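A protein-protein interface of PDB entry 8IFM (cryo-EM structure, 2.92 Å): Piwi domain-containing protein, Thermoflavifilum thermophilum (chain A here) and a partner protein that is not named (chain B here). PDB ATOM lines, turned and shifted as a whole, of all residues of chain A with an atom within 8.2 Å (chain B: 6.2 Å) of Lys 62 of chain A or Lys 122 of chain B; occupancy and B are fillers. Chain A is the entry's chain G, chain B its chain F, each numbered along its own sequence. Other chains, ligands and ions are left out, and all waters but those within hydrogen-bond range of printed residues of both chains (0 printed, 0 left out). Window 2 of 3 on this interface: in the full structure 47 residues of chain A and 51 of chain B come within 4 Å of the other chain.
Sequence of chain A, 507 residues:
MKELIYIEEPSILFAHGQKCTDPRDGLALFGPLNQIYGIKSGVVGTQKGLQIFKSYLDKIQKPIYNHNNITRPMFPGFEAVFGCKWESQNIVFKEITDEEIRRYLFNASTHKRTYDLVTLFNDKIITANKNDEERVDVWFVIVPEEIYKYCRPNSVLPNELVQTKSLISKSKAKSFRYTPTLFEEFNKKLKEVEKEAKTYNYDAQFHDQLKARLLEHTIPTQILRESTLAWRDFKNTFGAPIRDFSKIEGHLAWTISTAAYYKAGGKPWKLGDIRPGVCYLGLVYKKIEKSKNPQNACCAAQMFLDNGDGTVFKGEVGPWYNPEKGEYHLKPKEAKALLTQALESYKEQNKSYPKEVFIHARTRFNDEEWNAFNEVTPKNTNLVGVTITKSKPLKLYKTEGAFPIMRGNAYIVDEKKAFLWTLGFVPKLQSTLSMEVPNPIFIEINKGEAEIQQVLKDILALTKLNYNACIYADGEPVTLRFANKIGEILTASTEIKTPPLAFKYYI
OD1 of Asp 119 of chain B is in hydrogen-bond range of N of Lys 121 of chain B (3.2 Å). O of Phe 120 of chain B sits close to NE1 of Trp 124 of chain B (3.4 Å). The backbone carbonyl oxygen of Asp 58 of chain A sits at hydrogen-bond distance from the side-chain amino group of Lys 62 of chain A (3.3 Å). The side-chain carboxylate (OE1) of Glu 79 of chain A sits close to the side-chain amide oxygen (OE1) of Gln 61 of chain A (2.7 Å).
Among the printed residues, pairs that only touch across the chains: Gln 61 of chain A with Ser 123 of chain B (3.7 Å), Lys 62 of chain A with Lys 121 of chain B (3.9 Å), Lys 62 of chain A with Lys 122 of chain B (3.6 Å), Pro 63 of chain A with Trp 124 of chain B (3.3 Å), Met 74 of chain A with Trp 124 of chain B (3.8 Å), Pro 76 of chain A with Trp 124 of chain B (3.7 Å), Glu 79 of chain A with Ala 125 of chain B (3.4 Å) and Ala 80 of chain A with Ala 125 of chain B (3.4 Å).
Lys 62 of chain A touches just these residues of chain B: Lys 121 (3.9 Å) and Lys 122 (3.6 Å). Of the printed residues of chain A, Lys 122 of chain B touches Lys 62. Of the printed residues of chain B, Glu 79 of chain A touches Ala 125. Of the printed residues of chain A, Trp 124 of chain B touches Pro 63, Met 74 and Pro 76. The nearest printed residue of chain B that does not touch Pro 76 of chain A is Ala 125 of chain B (5.9 Å).
Of the 20 printed residues of chain A, 7 touch a printed residue of chain B. Printed residues of chain A that touch a printed residue of chain B: Gln 61, Lys 62, Pro 63, Met 74, Pro 76, Glu 79 and Ala 80. Among the printed residues, 8 pairs touch across the chains.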
ATOM      1  N   LYS A  54      26.168 -14.605  19.004  1.00  0.00           N
ATOM      2  CA  LYS A  54      25.823 -15.023  20.359  1.00  0.00           C
ATOM      3  C   LYS A  54      24.913 -14.006  21.035  1.00  0.00           C
ATOM      4  O   LYS A  54      23.960 -14.385  21.725  1.00  0.00           O
ATOM      5  CB  LYS A  54      27.097 -15.252  21.174  1.00  0.00           C
ATOM      6  CG  LYS A  54      27.469 -16.724  21.314  1.00  0.00           C
ATOM      7  CD  LYS A  54      28.615 -16.958  22.289  1.00  0.00           C
ATOM      8  CE  LYS A  54      29.698 -15.902  22.157  1.00  0.00           C
ATOM      9  NZ  LYS A  54      30.977 -16.352  22.776  1.00  0.00           N
ATOM     10  N   SER A  55      25.177 -12.711  20.838  1.00  0.00           N
ATOM     11  CA  SER A  55      24.304 -11.685  21.397  1.00  0.00           C
ATOM     12  C   SER A  55      22.909 -11.757  20.791  1.00  0.00           C
ATOM     13  O   SER A  55      21.906 -11.662  21.508  1.00  0.00           O
ATOM     14  CB  SER A  55      24.910 -10.300  21.174  1.00  0.00           C
ATOM     15  OG  SER A  55      24.491  -9.764  19.933  1.00  0.00           O
ATOM     16  N   TYR A  56      22.820 -11.937  19.472  1.00  0.00           N
ATOM     17  CA  TYR A  56      21.503 -12.027  18.851  1.00  0.00           C
ATOM     18  C   TYR A  56      20.776 -13.302  19.260  1.00  0.00           C
ATOM     19  O   TYR A  56      19.548 -13.300  19.381  1.00  0.00           O
ATOM     20  CB  TYR A  56      21.619 -11.944  17.330  1.00  0.00           C
ATOM     21  CG  TYR A  56      20.275 -11.835  16.644  1.00  0.00           C
ATOM     22  CD1 TYR A  56      19.633 -10.610  16.528  1.00  0.00           C
ATOM     23  CD2 TYR A  56      19.641 -12.958  16.128  1.00  0.00           C
ATOM     24  CE1 TYR A  56      18.404 -10.503  15.914  1.00  0.00           C
ATOM     25  CE2 TYR A  56      18.413 -12.858  15.510  1.00  0.00           C
ATOM     26  CZ  TYR A  56      17.801 -11.631  15.409  1.00  0.00           C
ATOM     27  OH  TYR A  56      16.577 -11.530  14.797  1.00  0.00           O
ATOM     28  N   LEU A  57      21.505 -14.396  19.478  1.00  0.00           N
ATOM     29  CA  LEU A  57      20.867 -15.625  19.929  1.00  0.00           C
ATOM     30  C   LEU A  57      20.431 -15.517  21.381  1.00  0.00           C
ATOM     31  O   LEU A  57      19.488 -16.197  21.799  1.00  0.00           O
ATOM     32  CB  LEU A  57      21.816 -16.807  19.733  1.00  0.00           C
ATOM     33  CG  LEU A  57      21.195 -18.193  19.891  1.00  0.00           C
ATOM     34  CD1 LEU A  57      19.821 -18.217  19.254  1.00  0.00           C
ATOM     35  CD2 LEU A  57      22.085 -19.258  19.275  1.00  0.00           C
ATOM     36  N   ASP A  58      21.125 -14.694  22.168  1.00  0.00           N
ATOM     37  CA  ASP A  58      20.649 -14.360  23.506  1.00  0.00           C
ATOM     38  C   ASP A  58      19.363 -13.547  23.429  1.00  0.00           C
ATOM     39  O   ASP A  58      18.419 -13.772  24.195  1.00  0.00           O
ATOM     40  CB  ASP A  58      21.731 -13.587  24.264  1.00  0.00           C
ATOM     41  CG  ASP A  58      22.646 -14.492  25.066  1.00  0.00           C
ATOM     42  OD1 ASP A  58      22.725 -15.700  24.736  1.00  0.00           O
ATOM     43  OD2 ASP A  58      23.300 -13.992  26.006  1.00  0.00           O
ATOM     44  N   LYS A  59      19.324 -12.580  22.509  1.00  0.00           N
ATOM     45  CA  LYS A  59      18.136 -11.747  22.332  1.00  0.00           C
ATOM     46  C   LYS A  59      16.945 -12.556  21.825  1.00  0.00           C
ATOM     47  O   LYS A  59      15.798 -12.254  22.172  1.00  0.00           O
ATOM     48  CB  LYS A  59      18.461 -10.589  21.384  1.00  0.00           C
ATOM     49  CG  LYS A  59      17.261  -9.925  20.736  1.00  0.00           C
ATOM     50  CD  LYS A  59      17.530  -8.451  20.475  1.00  0.00           C
ATOM     51  CE  LYS A  59      18.908  -8.226  19.874  1.00  0.00           C
ATOM     52  NZ  LYS A  59      18.941  -7.016  19.006  1.00  0.00           N
ATOM     53  N   ILE A  60      17.200 -13.586  21.015  1.00  0.00           N
ATOM     54  CA  ILE A  60      16.121 -14.418  20.482  1.00  0.00           C
ATOM     55  C   ILE A  60      15.359 -15.105  21.610  1.00  0.00           C
ATOM     56  O   ILE A  60      14.135 -15.268  21.541  1.00  0.00           O
ATOM     57  CB  ILE A  60      16.682 -15.441  19.473  1.00  0.00           C
ATOM     58  CG1 ILE A  60      16.840 -14.811  18.089  1.00  0.00           C
ATOM     59  CG2 ILE A  60      15.796 -16.671  19.378  1.00  0.00           C
ATOM     60  CD1 ILE A  60      17.489 -15.739  17.087  1.00  0.00           C
ATOM     61  N   GLN A  61      16.066 -15.512  22.668  1.00  0.00           N
ATOM     62  CA  GLN A  61      15.419 -16.236  23.758  1.00  0.00           C
ATOM     63  C   GLN A  61      14.317 -15.401  24.401  1.00  0.00           C
ATOM     64  O   GLN A  61      13.209 -15.895  24.646  1.00  0.00           O
ATOM     65  CB  GLN A  61      16.457 -16.645  24.803  1.00  0.00           C
ATOM     66  CG  GLN A  61      17.815 -16.990  24.233  1.00  0.00           C
ATOM     67  CD  GLN A  61      17.798 -18.263  23.414  1.00  0.00           C
ATOM     68  OE1 GLN A  61      17.401 -19.319  23.902  1.00  0.00           O
ATOM     69  NE2 GLN A  61      18.215 -18.166  22.161  1.00  0.00           N
ATOM     70  N   LYS A  62      14.602 -14.137  24.677  1.00  0.00           N
ATOM     71  CA  LYS A  62      13.602 -13.240  25.234  1.00  0.00           C
ATOM     72  C   LYS A  62      12.652 -12.794  24.131  1.00  0.00           C
ATOM     73  O   LYS A  62      13.088 -12.607  22.987  1.00  0.00           O
ATOM     74  CB  LYS A  62      14.264 -12.026  25.876  1.00  0.00           C
ATOM     75  CG  LYS A  62      15.373 -12.380  26.848  1.00  0.00           C
ATOM     76  CD  LYS A  62      16.432 -11.296  26.928  1.00  0.00           C
ATOM     77  CE  LYS A  62      17.759 -11.863  27.399  1.00  0.00           C
ATOM     78  NZ  LYS A  62      18.892 -11.480  26.516  1.00  0.00           N
ATOM     79  N   PRO A  63      11.357 -12.661  24.414  1.00  0.00           N
ATOM     80  CA  PRO A  63      10.427 -12.180  23.389  1.00  0.00           C
ATOM     81  C   PRO A  63      10.810 -10.787  22.917  1.00  0.00           C
ATOM     82  O   PRO A  63      11.250  -9.946  23.700  1.00  0.00           O
ATOM     83  CB  PRO A  63       9.082 -12.174  24.125  1.00  0.00           C
ATOM     84  CG  PRO A  63       9.518 -12.030  25.560  1.00  0.00           C
ATOM     85  CD  PRO A  63      10.600 -13.047  25.608  1.00  0.00           C
ATOM     86  N   ILE A  64      10.644 -10.553  21.618  1.00  0.00           N
ATOM     87  CA  ILE A  64      11.013  -9.289  21.001  1.00  0.00           C
ATOM     88  C   ILE A  64       9.782  -8.717  20.307  1.00  0.00           C
ATOM     89  O   ILE A  64       8.892  -9.446  19.861  1.00  0.00           O
ATOM     90  CB  ILE A  64      12.193  -9.460  20.024  1.00  0.00           C
ATOM     91  CG1 ILE A  64      12.654  -8.109  19.474  1.00  0.00           C
ATOM     92  CG2 ILE A  64      11.822 -10.427  18.916  1.00  0.00           C
ATOM     93  CD1 ILE A  64      13.805  -7.506  20.246  1.00  0.00           C
ATOM     94  N   TYR A  65       9.744  -7.390  20.217  1.00  0.00           N
ATOM     95  CA  TYR A  65       8.554  -6.651  19.816  1.00  0.00           C
ATOM     96  C   TYR A  65       8.763  -5.982  18.464  1.00  0.00           C
ATOM     97  O   TYR A  65       9.806  -5.367  18.225  1.00  0.00           O
ATOM     98  CB  TYR A  65       8.206  -5.584  20.856  1.00  0.00           C
ATOM     99  CG  TYR A  65       7.651  -6.127  22.150  1.00  0.00           C
ATOM    100  CD1 TYR A  65       6.472  -6.856  22.176  1.00  0.00           C
ATOM    101  CD2 TYR A  65       8.311  -5.905  23.351  1.00  0.00           C
ATOM    102  CE1 TYR A  65       5.967  -7.347  23.359  1.00  0.00           C
ATOM    103  CE2 TYR A  65       7.813  -6.395  24.538  1.00  0.00           C
ATOM    104  CZ  TYR A  65       6.641  -7.117  24.537  1.00  0.00           C
ATOM    105  OH  TYR A  65       6.139  -7.608  25.718  1.00  0.00           O
ATOM    106  N   MET A  74       4.286 -10.653  17.397  1.00  0.00           N
ATOM    107  CA  MET A  74       5.503 -10.706  18.187  1.00  0.00           C
ATOM    108  C   MET A  74       6.206 -12.046  18.008  1.00  0.00           C
ATOM    109  O   MET A  74       5.642 -13.019  17.501  1.00  0.00           O
ATOM    110  CB  MET A  74       5.200 -10.516  19.670  1.00  0.00           C
ATOM    111  CG  MET A  74       4.267 -11.589  20.217  1.00  0.00           C
ATOM    112  SD  MET A  74       4.619 -12.064  21.919  1.00  0.00           S
ATOM    113  CE  MET A  74       5.085 -10.495  22.625  1.00  0.00           C
ATOM    114  N   PHE A  75       7.456 -12.092  18.458  1.00  0.00           N
ATOM    115  CA  PHE A  75       8.147 -13.359  18.609  1.00  0.00           C
ATOM    116  C   PHE A  75       8.109 -13.748  20.075  1.00  0.00           C
ATOM    117  O   PHE A  75       8.759 -13.087  20.897  1.00  0.00           O
ATOM    118  CB  PHE A  75       9.589 -13.267  18.119  1.00  0.00           C
ATOM    119  CG  PHE A  75      10.255 -14.601  17.979  1.00  0.00           C
ATOM    120  CD1 PHE A  75       9.578 -15.668  17.418  1.00  0.00           C
ATOM    121  CD2 PHE A  75      11.549 -14.796  18.423  1.00  0.00           C
ATOM    122  CE1 PHE A  75      10.177 -16.902  17.295  1.00  0.00           C
ATOM    123  CE2 PHE A  75      12.154 -16.029  18.301  1.00  0.00           C
ATOM    124  CZ  PHE A  75      11.464 -17.083  17.736  1.00  0.00           C
ATOM    125  N   PRO A  76       7.363 -14.786  20.454  1.00  0.00           N
ATOM    126  CA  PRO A  76       7.332 -15.190  21.869  1.00  0.00           C
ATOM    127  C   PRO A  76       8.692 -15.591  22.407  1.00  0.00           C
ATOM    128  O   PRO A  76       8.966 -15.385  23.594  1.00  0.00           O
ATOM    129  CB  PRO A  76       6.350 -16.373  21.875  1.00  0.00           C
ATOM    130  CG  PRO A  76       5.607 -16.290  20.585  1.00  0.00           C
ATOM    131  CD  PRO A  76       6.534 -15.656  19.606  1.00  0.00           C
ATOM    132  N   GLY A  77       9.560 -16.131  21.563  1.00  0.00           N
ATOM    133  CA  GLY A  77      10.844 -16.659  21.992  1.00  0.00           C
ATOM    134  C   GLY A  77      10.983 -18.043  21.397  1.00  0.00           C
ATOM    135  O   GLY A  77      10.005 -18.778  21.240  1.00  0.00           O
ATOM    136  N   PHE A  78      12.224 -18.414  21.075  1.00  0.00           N
ATOM    137  CA  PHE A  78      12.454 -19.604  20.262  1.00  0.00           C
ATOM    138  C   PHE A  78      11.898 -20.858  20.925  1.00  0.00           C
ATOM    139  O   PHE A  78      11.233 -21.674  20.276  1.00  0.00           O
ATOM    140  CB  PHE A  78      13.945 -19.767  19.977  1.00  0.00           C
ATOM    141  CG  PHE A  78      14.239 -20.726  18.867  1.00  0.00           C
ATOM    142  CD1 PHE A  78      14.310 -22.085  19.106  1.00  0.00           C
ATOM    143  CD2 PHE A  78      14.417 -20.271  17.576  1.00  0.00           C
ATOM    144  CE1 PHE A  78      14.569 -22.965  18.083  1.00  0.00           C
ATOM    145  CE2 PHE A  78      14.673 -21.150  16.548  1.00  0.00           C
ATOM    146  CZ  PHE A  78      14.749 -22.496  16.802  1.00  0.00           C
ATOM    147  N   GLU A  79      12.169 -21.038  22.217  1.00  0.00           N
ATOM    148  CA  GLU A  79      11.640 -22.209  22.907  1.00  0.00           C
ATOM    149  C   GLU A  79      10.137 -22.094  23.128  1.00  0.00           C
ATOM    150  O   GLU A  79       9.445 -23.115  23.206  1.00  0.00           O
ATOM    151  CB  GLU A  79      12.360 -22.436  24.242  1.00  0.00           C
ATOM    152  CG  GLU A  79      13.894 -22.413  24.214  1.00  0.00           C
ATOM    153  CD  GLU A  79      14.490 -21.064  23.864  1.00  0.00           C
ATOM    154  OE1 GLU A  79      15.490 -21.041  23.117  1.00  0.00           O
ATOM    155  OE2 GLU A  79      13.968 -20.034  24.340  1.00  0.00           O
ATOM    156  N   ALA A  80       9.620 -20.869  23.237  1.00  0.00           N
ATOM    157  CA  ALA A  80       8.179 -20.684  23.369  1.00  0.00           C
ATOM    158  C   ALA A  80       7.447 -21.161  22.121  1.00  0.00           C
ATOM    159  O   ALA A  80       6.386 -21.788  22.215  1.00  0.00           O
ATOM    160  CB  ALA A  80       7.860 -19.217  23.654  1.00  0.00           C
ATOM    161  N   ALA A 253      13.369 -11.691  13.918  1.00  0.00           N
ATOM    162  CA  ALA A 253      13.599 -12.836  14.792  1.00  0.00           C
ATOM    163  C   ALA A 253      12.757 -14.031  14.365  1.00  0.00           C
ATOM    164  O   ALA A 253      13.249 -15.161  14.304  1.00  0.00           O
ATOM    165  CB  ALA A 253      13.307 -12.454  16.243  1.00  0.00           C
ATOM    166  N   ILE B  99       8.076 -10.300  34.245  1.00  0.00           N
ATOM    167  CA  ILE B  99       8.415 -10.454  32.835  1.00  0.00           C
ATOM    168  C   ILE B  99       9.319  -9.329  32.350  1.00  0.00           C
ATOM    169  O   ILE B  99       9.844  -9.387  31.233  1.00  0.00           O
ATOM    170  CB  ILE B  99       7.144 -10.520  31.968  1.00  0.00           C
ATOM    171  CG1 ILE B  99       6.594  -9.112  31.731  1.00  0.00           C
ATOM    172  CG2 ILE B  99       6.098 -11.405  32.612  1.00  0.00           C
ATOM    173  CD1 ILE B  99       5.202  -9.088  31.144  1.00  0.00           C
ATOM    174  N   GLU B 101      12.601  -6.835  32.417  1.00  0.00           N
ATOM    175  CA  GLU B 101      13.994  -6.733  32.837  1.00  0.00           C
ATOM    176  C   GLU B 101      14.263  -5.449  33.611  1.00  0.00           C
ATOM    177  O   GLU B 101      15.111  -5.436  34.510  1.00  0.00           O
ATOM    178  CB  GLU B 101      14.906  -6.817  31.613  1.00  0.00           C
ATOM    179  CG  GLU B 101      14.524  -5.848  30.502  1.00  0.00           C
ATOM    180  CD  GLU B 101      14.969  -6.317  29.131  1.00  0.00           C
ATOM    181  OE1 GLU B 101      15.743  -7.294  29.058  1.00  0.00           O
ATOM    182  OE2 GLU B 101      14.543  -5.709  28.127  1.00  0.00           O
ATOM    183  N   ASP B 119       9.887 -16.701  36.981  1.00  0.00           N
ATOM    184  CA  ASP B 119      10.732 -15.860  36.141  1.00  0.00           C
ATOM    185  C   ASP B 119      10.340 -16.021  34.677  1.00  0.00           C
ATOM    186  O   ASP B 119      10.622 -17.053  34.059  1.00  0.00           O
ATOM    187  CB  ASP B 119      12.201 -16.216  36.356  1.00  0.00           C
ATOM    188  CG  ASP B 119      13.131 -15.067  36.025  1.00  0.00           C
ATOM    189  OD1 ASP B 119      12.622 -13.977  35.699  1.00  0.00           O
ATOM    190  OD2 ASP B 119      14.365 -15.250  36.095  1.00  0.00           O
ATOM    191  N   PHE B 120       9.686 -15.000  34.122  1.00  0.00           N
ATOM    192  CA  PHE B 120       9.502 -14.861  32.682  1.00  0.00           C
ATOM    193  C   PHE B 120      10.451 -13.839  32.072  1.00  0.00           C
ATOM    194  O   PHE B 120      10.265 -13.459  30.911  1.00  0.00           O
ATOM    195  CB  PHE B 120       8.063 -14.463  32.337  1.00  0.00           C
ATOM    196  CG  PHE B 120       7.073 -15.590  32.397  1.00  0.00           C
ATOM    197  CD1 PHE B 120       6.704 -16.159  33.601  1.00  0.00           C
ATOM    198  CD2 PHE B 120       6.502 -16.069  31.231  1.00  0.00           C
ATOM    199  CE1 PHE B 120       5.778 -17.187  33.634  1.00  0.00           C
ATOM    200  CE2 PHE B 120       5.585 -17.096  31.262  1.00  0.00           C
ATOM    201  CZ  PHE B 120       5.222 -17.656  32.466  1.00  0.00           C
ATOM    202  N   LYS B 121      11.450 -13.372  32.824  1.00  0.00           N
ATOM    203  CA  LYS B 121      12.346 -12.345  32.298  1.00  0.00           C
ATOM    204  C   LYS B 121      13.084 -12.838  31.062  1.00  0.00           C
ATOM    205  O   LYS B 121      13.251 -12.091  30.091  1.00  0.00           O
ATOM    206  CB  LYS B 121      13.337 -11.902  33.374  1.00  0.00           C
ATOM    207  CG  LYS B 121      12.973 -10.595  34.061  1.00  0.00           C
ATOM    208  CD  LYS B 121      12.330 -10.834  35.416  1.00  0.00           C
ATOM    209  CE  LYS B 121      12.707  -9.739  36.400  1.00  0.00           C
ATOM    210  NZ  LYS B 121      11.883  -9.778  37.638  1.00  0.00           N
ATOM    211  N   LYS B 122      13.536 -14.087  31.081  1.00  0.00           N
ATOM    212  CA  LYS B 122      14.156 -14.723  29.929  1.00  0.00           C
ATOM    213  C   LYS B 122      13.410 -16.010  29.610  1.00  0.00           C
ATOM    214  O   LYS B 122      12.993 -16.732  30.520  1.00  0.00           O
ATOM    215  CB  LYS B 122      15.631 -15.038  30.194  1.00  0.00           C
ATOM    216  CG  LYS B 122      16.544 -13.826  30.211  1.00  0.00           C
ATOM    217  CD  LYS B 122      17.391 -13.804  31.475  1.00  0.00           C
ATOM    218  CE  LYS B 122      16.677 -13.096  32.613  1.00  0.00           C
ATOM    219  NZ  LYS B 122      16.855 -11.619  32.558  1.00  0.00           N
ATOM    220  N   SER B 123      13.243 -16.295  28.318  1.00  0.00           N
ATOM    221  CA  SER B 123      12.766 -17.597  27.849  1.00  0.00           C
ATOM    222  C   SER B 123      11.392 -17.932  28.439  1.00  0.00           C
ATOM    223  O   SER B 123      11.245 -18.805  29.298  1.00  0.00           O
ATOM    224  CB  SER B 123      13.786 -18.698  28.162  1.00  0.00           C
ATOM    225  OG  SER B 123      13.869 -18.940  29.552  1.00  0.00           O
ATOM    226  N   TRP B 124      10.390 -17.186  27.964  1.00  0.00           N
ATOM    227  CA  TRP B 124       8.990 -17.397  28.330  1.00  0.00           C
ATOM    228  C   TRP B 124       8.597 -18.869  28.380  1.00  0.00           C
ATOM    229  O   TRP B 124       7.694 -19.244  29.133  1.00  0.00           O
ATOM    230  CB  TRP B 124       8.066 -16.684  27.339  1.00  0.00           C
ATOM    231  CG  TRP B 124       7.826 -15.239  27.612  1.00  0.00           C
ATOM    232  CD1 TRP B 124       8.388 -14.481  28.595  1.00  0.00           C
ATOM    233  CD2 TRP B 124       6.950 -14.370  26.887  1.00  0.00           C
ATOM    234  NE1 TRP B 124       7.915 -13.193  28.528  1.00  0.00           N
ATOM    235  CE2 TRP B 124       7.029 -13.101  27.486  1.00  0.00           C
ATOM    236  CE3 TRP B 124       6.107 -14.545  25.786  1.00  0.00           C
ATOM    237  CZ2 TRP B 124       6.300 -12.011  27.021  1.00  0.00           C
ATOM    238  CZ3 TRP B 124       5.381 -13.465  25.327  1.00  0.00           C
ATOM    239  CH2 TRP B 124       5.484 -12.213  25.942  1.00  0.00           C
ATOM    240  N   ALA B 125       9.250 -19.706  27.573  1.00  0.00           N
ATOM    241  CA  ALA B 125       8.975 -21.137  27.626  1.00  0.00           C
ATOM    242  C   ALA B 125       9.355 -21.727  28.977  1.00  0.00           C
ATOM    243  O   ALA B 125       8.621 -22.563  29.519  1.00  0.00           O
ATOM    244  CB  ALA B 125       9.716 -21.857  26.504  1.00  0.00           C
ATOM    245  N   LYS B 126      10.494 -21.313  29.539  1.00  0.00           N
ATOM    246  CA  LYS B 126      10.877 -21.832  30.848  1.00  0.00           C
ATOM    247  C   LYS B 126       9.915 -21.347  31.927  1.00  0.00           C
ATOM    248  O   LYS B 126       9.584 -22.099  32.850  1.00  0.00           O
ATOM    249  CB  LYS B 126      12.322 -21.448  31.182  1.00  0.00           C
ATOM    250  CG  LYS B 126      12.487 -20.387  32.265  1.00  0.00           C
ATOM    251  CD  LYS B 126      13.952 -20.052  32.504  1.00  0.00           C
ATOM    252  CE  LYS B 126      14.137 -18.582  32.836  1.00  0.00           C
ATOM    253  NZ  LYS B 126      15.559 -18.254  33.134  1.00  0.00           N
ATOM    254  N   GLY B 127       9.439 -20.105  31.818  1.00  0.00           N
ATOM    255  CA  GLY B 127       8.448 -19.620  32.765  1.00  0.00           C
ATOM    256  C   GLY B 127       7.135 -20.373  32.665  1.00  0.00           C
ATOM    257  O   GLY B 127       6.513 -20.694  33.681  1.00  0.00           O
